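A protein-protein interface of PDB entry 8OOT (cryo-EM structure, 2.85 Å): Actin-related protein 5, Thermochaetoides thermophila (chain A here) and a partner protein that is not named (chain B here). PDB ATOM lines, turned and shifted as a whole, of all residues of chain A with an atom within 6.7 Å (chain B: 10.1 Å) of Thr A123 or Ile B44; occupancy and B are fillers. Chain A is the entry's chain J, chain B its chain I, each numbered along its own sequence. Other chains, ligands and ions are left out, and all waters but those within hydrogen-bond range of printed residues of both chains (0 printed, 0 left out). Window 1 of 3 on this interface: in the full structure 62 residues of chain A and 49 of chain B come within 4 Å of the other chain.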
ATOM      1  N   SER A  65      13.843  27.623 -26.476  1.00  0.00           N
ATOM      2  CA  SER A  65      14.752  26.528 -26.149  1.00  0.00           C
ATOM      3  C   SER A  65      14.479  25.254 -26.937  1.00  0.00           C
ATOM      4  O   SER A  65      15.389  24.434 -27.094  1.00  0.00           O
ATOM      5  CB  SER A  65      14.677  26.215 -24.655  1.00  0.00           C
ATOM      6  OG  SER A  65      14.821  27.390 -23.880  1.00  0.00           O
ATOM      7  N   PHE A 119      21.302  26.312 -24.533  1.00  0.00           N
ATOM      8  CA  PHE A 119      20.611  26.454 -23.264  1.00  0.00           C
ATOM      9  C   PHE A 119      21.143  25.460 -22.242  1.00  0.00           C
ATOM     10  O   PHE A 119      21.516  24.334 -22.576  1.00  0.00           O
ATOM     11  CB  PHE A 119      19.107  26.258 -23.448  1.00  0.00           C
ATOM     12  CG  PHE A 119      18.457  27.329 -24.270  1.00  0.00           C
ATOM     13  CD1 PHE A 119      18.461  27.262 -25.650  1.00  0.00           C
ATOM     14  CD2 PHE A 119      17.843  28.407 -23.661  1.00  0.00           C
ATOM     15  CE1 PHE A 119      17.866  28.251 -26.406  1.00  0.00           C
ATOM     16  CE2 PHE A 119      17.243  29.395 -24.412  1.00  0.00           C
ATOM     17  CZ  PHE A 119      17.257  29.317 -25.786  1.00  0.00           C
ATOM     18  N   GLU A 120      21.173  25.893 -20.986  1.00  0.00           N
ATOM     19  CA  GLU A 120      21.384  24.970 -19.880  1.00  0.00           C
ATOM     20  C   GLU A 120      20.177  24.051 -19.754  1.00  0.00           C
ATOM     21  O   GLU A 120      19.045  24.522 -19.607  1.00  0.00           O
ATOM     22  CB  GLU A 120      21.616  25.734 -18.582  1.00  0.00           C
ATOM     23  CG  GLU A 120      21.789  24.837 -17.376  1.00  0.00           C
ATOM     24  CD  GLU A 120      22.449  25.546 -16.216  1.00  0.00           C
ATOM     25  OE1 GLU A 120      23.292  26.433 -16.461  1.00  0.00           O
ATOM     26  OE2 GLU A 120      22.125  25.216 -15.058  1.00  0.00           O
ATOM     27  N   ALA A 121      20.422  22.744 -19.828  1.00  0.00           N
ATOM     28  CA  ALA A 121      19.349  21.778 -20.023  1.00  0.00           C
ATOM     29  C   ALA A 121      18.311  21.876 -18.913  1.00  0.00           C
ATOM     30  O   ALA A 121      18.645  21.889 -17.725  1.00  0.00           O
ATOM     31  CB  ALA A 121      19.925  20.364 -20.082  1.00  0.00           C
ATOM     32  N   GLY A 122      17.045  21.946 -19.313  1.00  0.00           N
ATOM     33  CA  GLY A 122      15.958  22.132 -18.374  1.00  0.00           C
ATOM     34  C   GLY A 122      15.817  23.526 -17.816  1.00  0.00           C
ATOM     35  O   GLY A 122      15.269  23.693 -16.722  1.00  0.00           O
ATOM     36  N   THR A 123      16.290  24.538 -18.538  1.00  0.00           N
ATOM     37  CA  THR A 123      16.110  25.927 -18.142  1.00  0.00           C
ATOM     38  C   THR A 123      15.857  26.763 -19.385  1.00  0.00           C
ATOM     39  O   THR A 123      16.158  26.352 -20.508  1.00  0.00           O
ATOM     40  CB  THR A 123      17.328  26.499 -17.395  1.00  0.00           C
ATOM     41  OG1 THR A 123      18.359  26.819 -18.338  1.00  0.00           O
ATOM     42  CG2 THR A 123      17.872  25.529 -16.358  1.00  0.00           C
ATOM     43  N   GLY A 124      15.288  27.942 -19.171  1.00  0.00           N
ATOM     44  CA  GLY A 124      15.022  28.878 -20.239  1.00  0.00           C
ATOM     45  C   GLY A 124      16.173  29.802 -20.561  1.00  0.00           C
ATOM     46  O   GLY A 124      16.016  30.708 -21.385  1.00  0.00           O
ATOM     47  N   ILE A 125      17.330  29.594 -19.943  1.00  0.00           N
ATOM     48  CA  ILE A 125      18.415  30.565 -19.936  1.00  0.00           C
ATOM     49  C   ILE A 125      19.491  30.105 -20.906  1.00  0.00           C
ATOM     50  O   ILE A 125      19.939  28.953 -20.847  1.00  0.00           O
ATOM     51  CB  ILE A 125      18.990  30.737 -18.521  1.00  0.00           C
ATOM     52  CG1 ILE A 125      17.883  31.122 -17.541  1.00  0.00           C
ATOM     53  CG2 ILE A 125      20.087  31.777 -18.519  1.00  0.00           C
ATOM     54  CD1 ILE A 125      17.214  32.431 -17.861  1.00  0.00           C
ATOM     55  N   VAL A 126      19.907  31.000 -21.802  1.00  0.00           N
ATOM     56  CA  VAL A 126      21.058  30.727 -22.652  1.00  0.00           C
ATOM     57  C   VAL A 126      22.325  30.759 -21.812  1.00  0.00           C
ATOM     58  O   VAL A 126      22.504  31.634 -20.954  1.00  0.00           O
ATOM     59  CB  VAL A 126      21.130  31.742 -23.805  1.00  0.00           C
ATOM     60  CG1 VAL A 126      22.366  31.499 -24.648  1.00  0.00           C
ATOM     61  CG2 VAL A 126      19.884  31.666 -24.658  1.00  0.00           C
ATOM     62  N   SER A 127      23.215  29.796 -22.049  1.00  0.00           N
ATOM     63  CA  SER A 127      24.471  29.728 -21.309  1.00  0.00           C
ATOM     64  C   SER A 127      25.667  29.277 -22.132  1.00  0.00           C
ATOM     65  O   SER A 127      26.797  29.599 -21.751  1.00  0.00           O
ATOM     66  CB  SER A 127      24.326  28.798 -20.099  1.00  0.00           C
ATOM     67  OG  SER A 127      24.093  27.466 -20.513  1.00  0.00           O
ATOM     68  N   LEU A 165      18.175  36.350 -16.661  1.00  0.00           N
ATOM     69  CA  LEU A 165      19.229  36.839 -15.782  1.00  0.00           C
ATOM     70  C   LEU A 165      19.986  37.997 -16.431  1.00  0.00           C
ATOM     71  O   LEU A 165      20.203  37.996 -17.646  1.00  0.00           O
ATOM     72  CB  LEU A 165      20.199  35.711 -15.441  1.00  0.00           C
ATOM     73  CG  LEU A 165      19.584  34.517 -14.714  1.00  0.00           C
ATOM     74  CD1 LEU A 165      20.597  33.400 -14.565  1.00  0.00           C
ATOM     75  CD2 LEU A 165      19.070  34.948 -13.354  1.00  0.00           C
ATOM     76  N   SER A 168      22.961  37.062 -18.534  1.00  0.00           N
ATOM     77  CA  SER A 168      22.565  36.458 -19.801  1.00  0.00           C
ATOM     78  C   SER A 168      22.102  37.513 -20.795  1.00  0.00           C
ATOM     79  O   SER A 168      22.411  37.427 -21.989  1.00  0.00           O
ATOM     80  CB  SER A 168      21.470  35.422 -19.564  1.00  0.00           C
ATOM     81  OG  SER A 168      21.910  34.433 -18.652  1.00  0.00           O
ATOM     82  N   TYR A 210       8.670  24.178 -23.395  1.00  0.00           N
ATOM     83  CA  TYR A 210       9.758  23.210 -23.320  1.00  0.00           C
ATOM     84  C   TYR A 210      10.586  23.393 -22.052  1.00  0.00           C
ATOM     85  O   TYR A 210      10.915  22.416 -21.372  1.00  0.00           O
ATOM     86  CB  TYR A 210      10.623  23.343 -24.572  1.00  0.00           C
ATOM     87  CG  TYR A 210      11.764  22.363 -24.698  1.00  0.00           C
ATOM     88  CD1 TYR A 210      13.029  22.667 -24.216  1.00  0.00           C
ATOM     89  CD2 TYR A 210      11.586  21.156 -25.355  1.00  0.00           C
ATOM     90  CE1 TYR A 210      14.060  21.761 -24.319  1.00  0.00           C
ATOM     91  CE2 TYR A 210      12.619  20.260 -25.493  1.00  0.00           C
ATOM     92  CZ  TYR A 210      13.853  20.562 -24.965  1.00  0.00           C
ATOM     93  OH  TYR A 210      14.893  19.683 -25.136  1.00  0.00           O
ATOM     94  N   SER A 211      10.929  24.636 -21.710  1.00  0.00           N
ATOM     95  CA  SER A 211      11.846  24.862 -20.598  1.00  0.00           C
ATOM     96  C   SER A 211      11.168  24.828 -19.232  1.00  0.00           C
ATOM     97  O   SER A 211      11.805  24.440 -18.247  1.00  0.00           O
ATOM     98  CB  SER A 211      12.561  26.201 -20.776  1.00  0.00           C
ATOM     99  OG  SER A 211      11.641  27.278 -20.716  1.00  0.00           O
ATOM    100  N   ALA A 212       9.902  25.222 -19.141  1.00  0.00           N
ATOM    101  CA  ALA A 212       9.319  25.610 -17.857  1.00  0.00           C
ATOM    102  C   ALA A 212       7.809  25.726 -18.020  1.00  0.00           C
ATOM    103  O   ALA A 212       7.269  25.582 -19.120  1.00  0.00           O
ATOM    104  CB  ALA A 212       9.926  26.911 -17.336  1.00  0.00           C
ATOM    105  N   TRP A 236      10.615  19.569 -21.884  1.00  0.00           N
ATOM    106  CA  TRP A 236      11.900  18.890 -21.734  1.00  0.00           C
ATOM    107  C   TRP A 236      11.880  17.912 -20.566  1.00  0.00           C
ATOM    108  O   TRP A 236      12.323  16.767 -20.694  1.00  0.00           O
ATOM    109  CB  TRP A 236      13.012  19.913 -21.527  1.00  0.00           C
ATOM    110  CG  TRP A 236      14.357  19.290 -21.342  1.00  0.00           C
ATOM    111  CD1 TRP A 236      15.196  18.857 -22.322  1.00  0.00           C
ATOM    112  CD2 TRP A 236      14.986  18.953 -20.102  1.00  0.00           C
ATOM    113  NE1 TRP A 236      16.329  18.317 -21.772  1.00  0.00           N
ATOM    114  CE2 TRP A 236      16.223  18.359 -20.409  1.00  0.00           C
ATOM    115  CE3 TRP A 236      14.628  19.107 -18.760  1.00  0.00           C
ATOM    116  CZ2 TRP A 236      17.105  17.923 -19.427  1.00  0.00           C
ATOM    117  CZ3 TRP A 236      15.508  18.679 -17.787  1.00  0.00           C
ATOM    118  CH2 TRP A 236      16.730  18.090 -18.124  1.00  0.00           C
ATOM    119  N   HIS A 237      11.377  18.358 -19.415  1.00  0.00           N
ATOM    120  CA  HIS A 237      11.305  17.505 -18.234  1.00  0.00           C
ATOM    121  C   HIS A 237      10.418  16.287 -18.460  1.00  0.00           C
ATOM    122  O   HIS A 237      10.705  15.198 -17.951  1.00  0.00           O
ATOM    123  CB  HIS A 237      10.803  18.320 -17.047  1.00  0.00           C
ATOM    124  CG  HIS A 237      11.673  19.488 -16.708  1.00  0.00           C
ATOM    125  ND1 HIS A 237      12.591  19.461 -15.681  1.00  0.00           N
ATOM    126  CD2 HIS A 237      11.777  20.714 -17.273  1.00  0.00           C
ATOM    127  CE1 HIS A 237      13.213  20.624 -15.619  1.00  0.00           C
ATOM    128  NE2 HIS A 237      12.739  21.401 -16.575  1.00  0.00           N
ATOM    129  N   ARG B  40      33.059  33.280 -20.871  1.00  0.00           N
ATOM    130  CA  ARG B  40      31.693  33.797 -20.832  1.00  0.00           C
ATOM    131  C   ARG B  40      30.651  32.711 -20.579  1.00  0.00           C
ATOM    132  O   ARG B  40      29.576  33.005 -20.043  1.00  0.00           O
ATOM    133  CB  ARG B  40      31.388  34.549 -22.128  1.00  0.00           C
ATOM    134  CG  ARG B  40      31.319  33.682 -23.366  1.00  0.00           C
ATOM    135  CD  ARG B  40      31.015  34.528 -24.583  1.00  0.00           C
ATOM    136  NE  ARG B  40      31.117  33.770 -25.821  1.00  0.00           N
ATOM    137  CZ  ARG B  40      30.657  34.189 -26.990  1.00  0.00           C
ATOM    138  NH1 ARG B  40      30.037  35.350 -27.111  1.00  0.00           N
ATOM    139  NH2 ARG B  40      30.820  33.423 -28.065  1.00  0.00           N
ATOM    140  N   ASN B  41      30.933  31.459 -20.945  1.00  0.00           N
ATOM    141  CA  ASN B  41      29.967  30.370 -20.775  1.00  0.00           C
ATOM    142  C   ASN B  41      29.877  29.901 -19.319  1.00  0.00           C
ATOM    143  O   ASN B  41      30.192  28.764 -18.971  1.00  0.00           O
ATOM    144  CB  ASN B  41      30.313  29.214 -21.702  1.00  0.00           C
ATOM    145  CG  ASN B  41      30.167  29.576 -23.162  1.00  0.00           C
ATOM    146  OD1 ASN B  41      29.654  30.642 -23.498  1.00  0.00           O
ATOM    147  ND2 ASN B  41      30.608  28.686 -24.040  1.00  0.00           N
ATOM    148  N   LYS B  42      29.436  30.816 -18.460  1.00  0.00           N
ATOM    149  CA  LYS B  42      29.174  30.495 -17.064  1.00  0.00           C
ATOM    150  C   LYS B  42      27.886  29.686 -16.924  1.00  0.00           C
ATOM    151  O   LYS B  42      26.970  29.787 -17.745  1.00  0.00           O
ATOM    152  CB  LYS B  42      29.089  31.775 -16.241  1.00  0.00           C
ATOM    153  CG  LYS B  42      30.347  32.609 -16.334  1.00  0.00           C
ATOM    154  CD  LYS B  42      30.297  33.817 -15.431  1.00  0.00           C
ATOM    155  CE  LYS B  42      31.540  34.667 -15.616  1.00  0.00           C
ATOM    156  NZ  LYS B  42      31.586  35.811 -14.670  1.00  0.00           N
ATOM    157  N   THR B  43      27.822  28.870 -15.873  1.00  0.00           N
ATOM    158  CA  THR B  43      26.581  28.194 -15.521  1.00  0.00           C
ATOM    159  C   THR B  43      25.644  29.125 -14.753  1.00  0.00           C
ATOM    160  O   THR B  43      26.061  30.122 -14.159  1.00  0.00           O
ATOM    161  CB  THR B  43      26.861  26.944 -14.690  1.00  0.00           C
ATOM    162  OG1 THR B  43      27.489  27.317 -13.457  1.00  0.00           O
ATOM    163  CG2 THR B  43      27.771  25.994 -15.448  1.00  0.00           C
ATOM    164  N   ILE B  44      24.354  28.775 -14.777  1.00  0.00           N
ATOM    165  CA  ILE B  44      23.346  29.505 -14.006  1.00  0.00           C
ATOM    166  C   ILE B  44      23.702  29.537 -12.525  1.00  0.00           C
ATOM    167  O   ILE B  44      23.531  30.563 -11.854  1.00  0.00           O
ATOM    168  CB  ILE B  44      21.954  28.886 -14.237  1.00  0.00           C
ATOM    169  CG1 ILE B  44      21.481  29.159 -15.663  1.00  0.00           C
ATOM    170  CG2 ILE B  44      20.952  29.422 -13.232  1.00  0.00           C
ATOM    171  CD1 ILE B  44      20.328  28.288 -16.091  1.00  0.00           C
ATOM    172  N   LYS B  45      24.196  28.419 -11.992  1.00  0.00           N
ATOM    173  CA  LYS B  45      24.656  28.388 -10.606  1.00  0.00           C
ATOM    174  C   LYS B  45      25.719  29.449 -10.353  1.00  0.00           C
ATOM    175  O   LYS B  45      25.679  30.161  -9.344  1.00  0.00           O
ATOM    176  CB  LYS B  45      25.186  26.996 -10.263  1.00  0.00           C
ATOM    177  CG  LYS B  45      25.642  26.845  -8.822  1.00  0.00           C
ATOM    178  CD  LYS B  45      26.148  25.439  -8.548  1.00  0.00           C
ATOM    179  CE  LYS B  45      26.749  25.330  -7.156  1.00  0.00           C
ATOM    180  NZ  LYS B  45      25.712  25.434  -6.093  1.00  0.00           N
ATOM    181  N   ALA B  46      26.686  29.563 -11.264  1.00  0.00           N
ATOM    182  CA  ALA B  46      27.717  30.589 -11.139  1.00  0.00           C
ATOM    183  C   ALA B  46      27.142  31.990 -11.318  1.00  0.00           C
ATOM    184  O   ALA B  46      27.483  32.906 -10.560  1.00  0.00           O
ATOM    185  CB  ALA B  46      28.834  30.334 -12.149  1.00  0.00           C
ATOM    186  N   ILE B  47      26.278  32.178 -12.317  1.00  0.00           N
ATOM    187  CA  ILE B  47      25.680  33.489 -12.562  1.00  0.00           C
ATOM    188  C   ILE B  47      24.894  33.963 -11.345  1.00  0.00           C
ATOM    189  O   ILE B  47      25.001  35.123 -10.930  1.00  0.00           O
ATOM    190  CB  ILE B  47      24.793  33.443 -13.818  1.00  0.00           C
ATOM    191  CG1 ILE B  47      25.642  33.193 -15.062  1.00  0.00           C
ATOM    192  CG2 ILE B  47      24.021  34.736 -13.966  1.00  0.00           C
ATOM    193  CD1 ILE B  47      24.848  32.700 -16.249  1.00  0.00           C
ATOM    194  N   LEU B  48      24.095  33.076 -10.751  1.00  0.00           N
ATOM    195  CA  LEU B  48      23.422  33.415  -9.500  1.00  0.00           C
ATOM    196  C   LEU B  48      24.427  33.717  -8.397  1.00  0.00           C
ATOM    197  O   LEU B  48      24.332  34.747  -7.720  1.00  0.00           O
ATOM    198  CB  LEU B  48      22.485  32.284  -9.078  1.00  0.00           C
ATOM    199  CG  LEU B  48      21.017  32.398  -9.493  1.00  0.00           C
ATOM    200  CD1 LEU B  48      20.873  32.630 -10.986  1.00  0.00           C
ATOM    201  CD2 LEU B  48      20.250  31.159  -9.067  1.00  0.00           C
ATOM    202  N   GLY B  49      25.391  32.821  -8.194  1.00  0.00           N
ATOM    203  CA  GLY B  49      26.345  32.996  -7.110  1.00  0.00           C
ATOM    204  C   GLY B  49      27.185  34.253  -7.224  1.00  0.00           C
ATOM    205  O   GLY B  49      27.668  34.773  -6.216  1.00  0.00           O
ATOM    206  N   GLU B  50      27.371  34.760  -8.444  1.00  0.00           N
ATOM    207  CA  GLU B  50      28.050  36.038  -8.627  1.00  0.00           C
ATOM    208  C   GLU B  50      27.221  37.239  -8.189  1.00  0.00           C
ATOM    209  O   GLU B  50      27.771  38.341  -8.106  1.00  0.00           O
ATOM    210  CB  GLU B  50      28.448  36.208 -10.092  1.00  0.00           C
ATOM    211  CG  GLU B  50      29.653  35.386 -10.497  1.00  0.00           C
ATOM    212  CD  GLU B  50      30.025  35.583 -11.950  1.00  0.00           C
ATOM    213  OE1 GLU B  50      29.420  36.457 -12.605  1.00  0.00           O
ATOM    214  OE2 GLU B  50      30.923  34.865 -12.436  1.00  0.00           O
ATOM    215  N   SER B  51      25.926  37.066  -7.915  1.00  0.00           N
ATOM    216  CA  SER B  51      25.119  38.206  -7.490  1.00  0.00           C
ATOM    217  C   SER B  51      25.576  38.727  -6.132  1.00  0.00           C
ATOM    218  O   SER B  51      25.558  39.938  -5.886  1.00  0.00           O
ATOM    219  CB  SER B  51      23.641  37.826  -7.451  1.00  0.00           C
ATOM    220  OG  SER B  51      23.252  37.177  -8.648  1.00  0.00           O
ATOM    221  N   GLN B  52      25.993  37.830  -5.246  1.00  0.00           N
ATOM    222  CA  GLN B  52      26.502  38.218  -3.938  1.00  0.00           C
ATOM    223  C   GLN B  52      27.929  38.746  -4.042  1.00  0.00           C
ATOM    224  O   GLN B  52      28.866  37.987  -4.288  1.00  0.00           O
ATOM    225  CB  GLN B  52      26.443  37.035  -2.968  1.00  0.00           C
ATOM    226  CG  GLN B  52      25.032  36.633  -2.561  1.00  0.00           C
ATOM    227  CD  GLN B  52      24.287  35.900  -3.659  1.00  0.00           C
ATOM    228  OE1 GLN B  52      24.888  35.435  -4.627  1.00  0.00           O
ATOM    229  NE2 GLN B  52      22.972  35.796  -3.514  1.00  0.00           N
ATOM    230  N   THR B 155      12.630  37.054 -10.461  1.00  0.00           N
ATOM    231  CA  THR B 155      14.064  37.278 -10.578  1.00  0.00           C
ATOM    232  C   THR B 155      14.827  35.986 -10.325  1.00  0.00           C
ATOM    233  O   THR B 155      15.860  35.985  -9.658  1.00  0.00           O
ATOM    234  CB  THR B 155      14.546  38.357  -9.601  1.00  0.00           C
ATOM    235  OG1 THR B 155      14.588  37.817  -8.276  1.00  0.00           O
ATOM    236  CG2 THR B 155      13.601  39.544  -9.621  1.00  0.00           C
ATOM    237  N   ASN B 156      14.295  34.886 -10.860  1.00  0.00           N
ATOM    238  CA  ASN B 156      14.572  33.539 -10.358  1.00  0.00           C
ATOM    239  C   ASN B 156      14.297  33.434  -8.857  1.00  0.00           C
ATOM    240  O   ASN B 156      14.996  32.741  -8.116  1.00  0.00           O
ATOM    241  CB  ASN B 156      15.997  33.108 -10.703  1.00  0.00           C
ATOM    242  CG  ASN B 156      16.145  32.718 -12.165  1.00  0.00           C
ATOM    243  OD1 ASN B 156      15.505  33.303 -13.038  1.00  0.00           O
ATOM    244  ND2 ASN B 156      16.976  31.721 -12.435  1.00  0.00           N
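OE1 of Glu A120 is in hydrogen-bond range of N of Ile B44, at 3.1 Å.
N of Ala B46 lies within hydrogen-bond range of OG1 of Thr B43, 3.2 Å away. O of Leu B48 sits at hydrogen-bond distance from OG of Ser B51 (2.8 Å). The backbone carbonyl oxygen of Glu A120 lies within hydrogen-bond range of the side-chain hydroxyl of Thr A123 (2.7 Å). The backbone carbonyl oxygen (O) of Ile A125 is in hydrogen-bond range of the backbone NH (N) of Glu A120 (3.3 Å). The backbone NH (N) of Glu A120 sits at hydrogen-bond distance from the side-chain hydroxyl (OG) of Ser A127. N of Ile A125 sits close to OG1 of Thr A123 (3.4 Å).
Among the printed residues, pairs that only touch across the chains: Glu A120 with Thr B43 (3.8 Å), Thr A123 with Ile B44 (3.3 Å), Ile A125 with Ile B44 (3.7 Å), Ser A127 with Asn B41 (3.4 Å), Ser A127 with Lys B42 (3.7 Å), Leu A165 with Ile B47 (3.7 Å), Leu A165 with Leu B48 (3.7 Å) and Leu A165 with Asn B156 (3.9 Å).
No residue of chain B comes within 4 Å of Ala A121. Of the printed residues of chain B, Thr A123 touches Ile B44 (3.3 Å). No residue of chain B comes within 4 Å of Gly A124. Of chain B, only Ile B44 comes within 4 Å of Ile A125. Of the printed residues of chain B, Ser A127 touches Asn B41 and Lys B42. No residue of chain B comes within 4 Å of Ser A211. Printed residues of chain A within 4 Å of Leu B48: Leu A165 (3.7 Å). Gly B49 touches none of the printed residues of chain A. Gln B52 touches none of the printed residues of chain A. Of the printed residues of chain A, Asn B156 touches Leu A165. The nearest residue of chain A that does not touch Ile B44 is Leu A165 (4.2 Å).
Of the 17 printed residues of chain A, 5 touch a printed residue of chain B. Printed residues of chain A that touch a printed residue of chain B: Glu A120, Thr A123, Ile A125, Ser A127 and Leu A165. Hydrophobic or aromatic side chains of chain A within 4 Å of the printed part of chain B: Ile A125 and Leu A165. Along chain A the printed residues that touch a printed residue of chain B span positions 120 to 165. Of the 15 printed residues of chain B, 7 touch a printed residue of chain A. Among the printed residues, no Asp or Glu carboxylate lies within 4 Å of a Lys or Arg side-chain nitrogen of the other chain.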
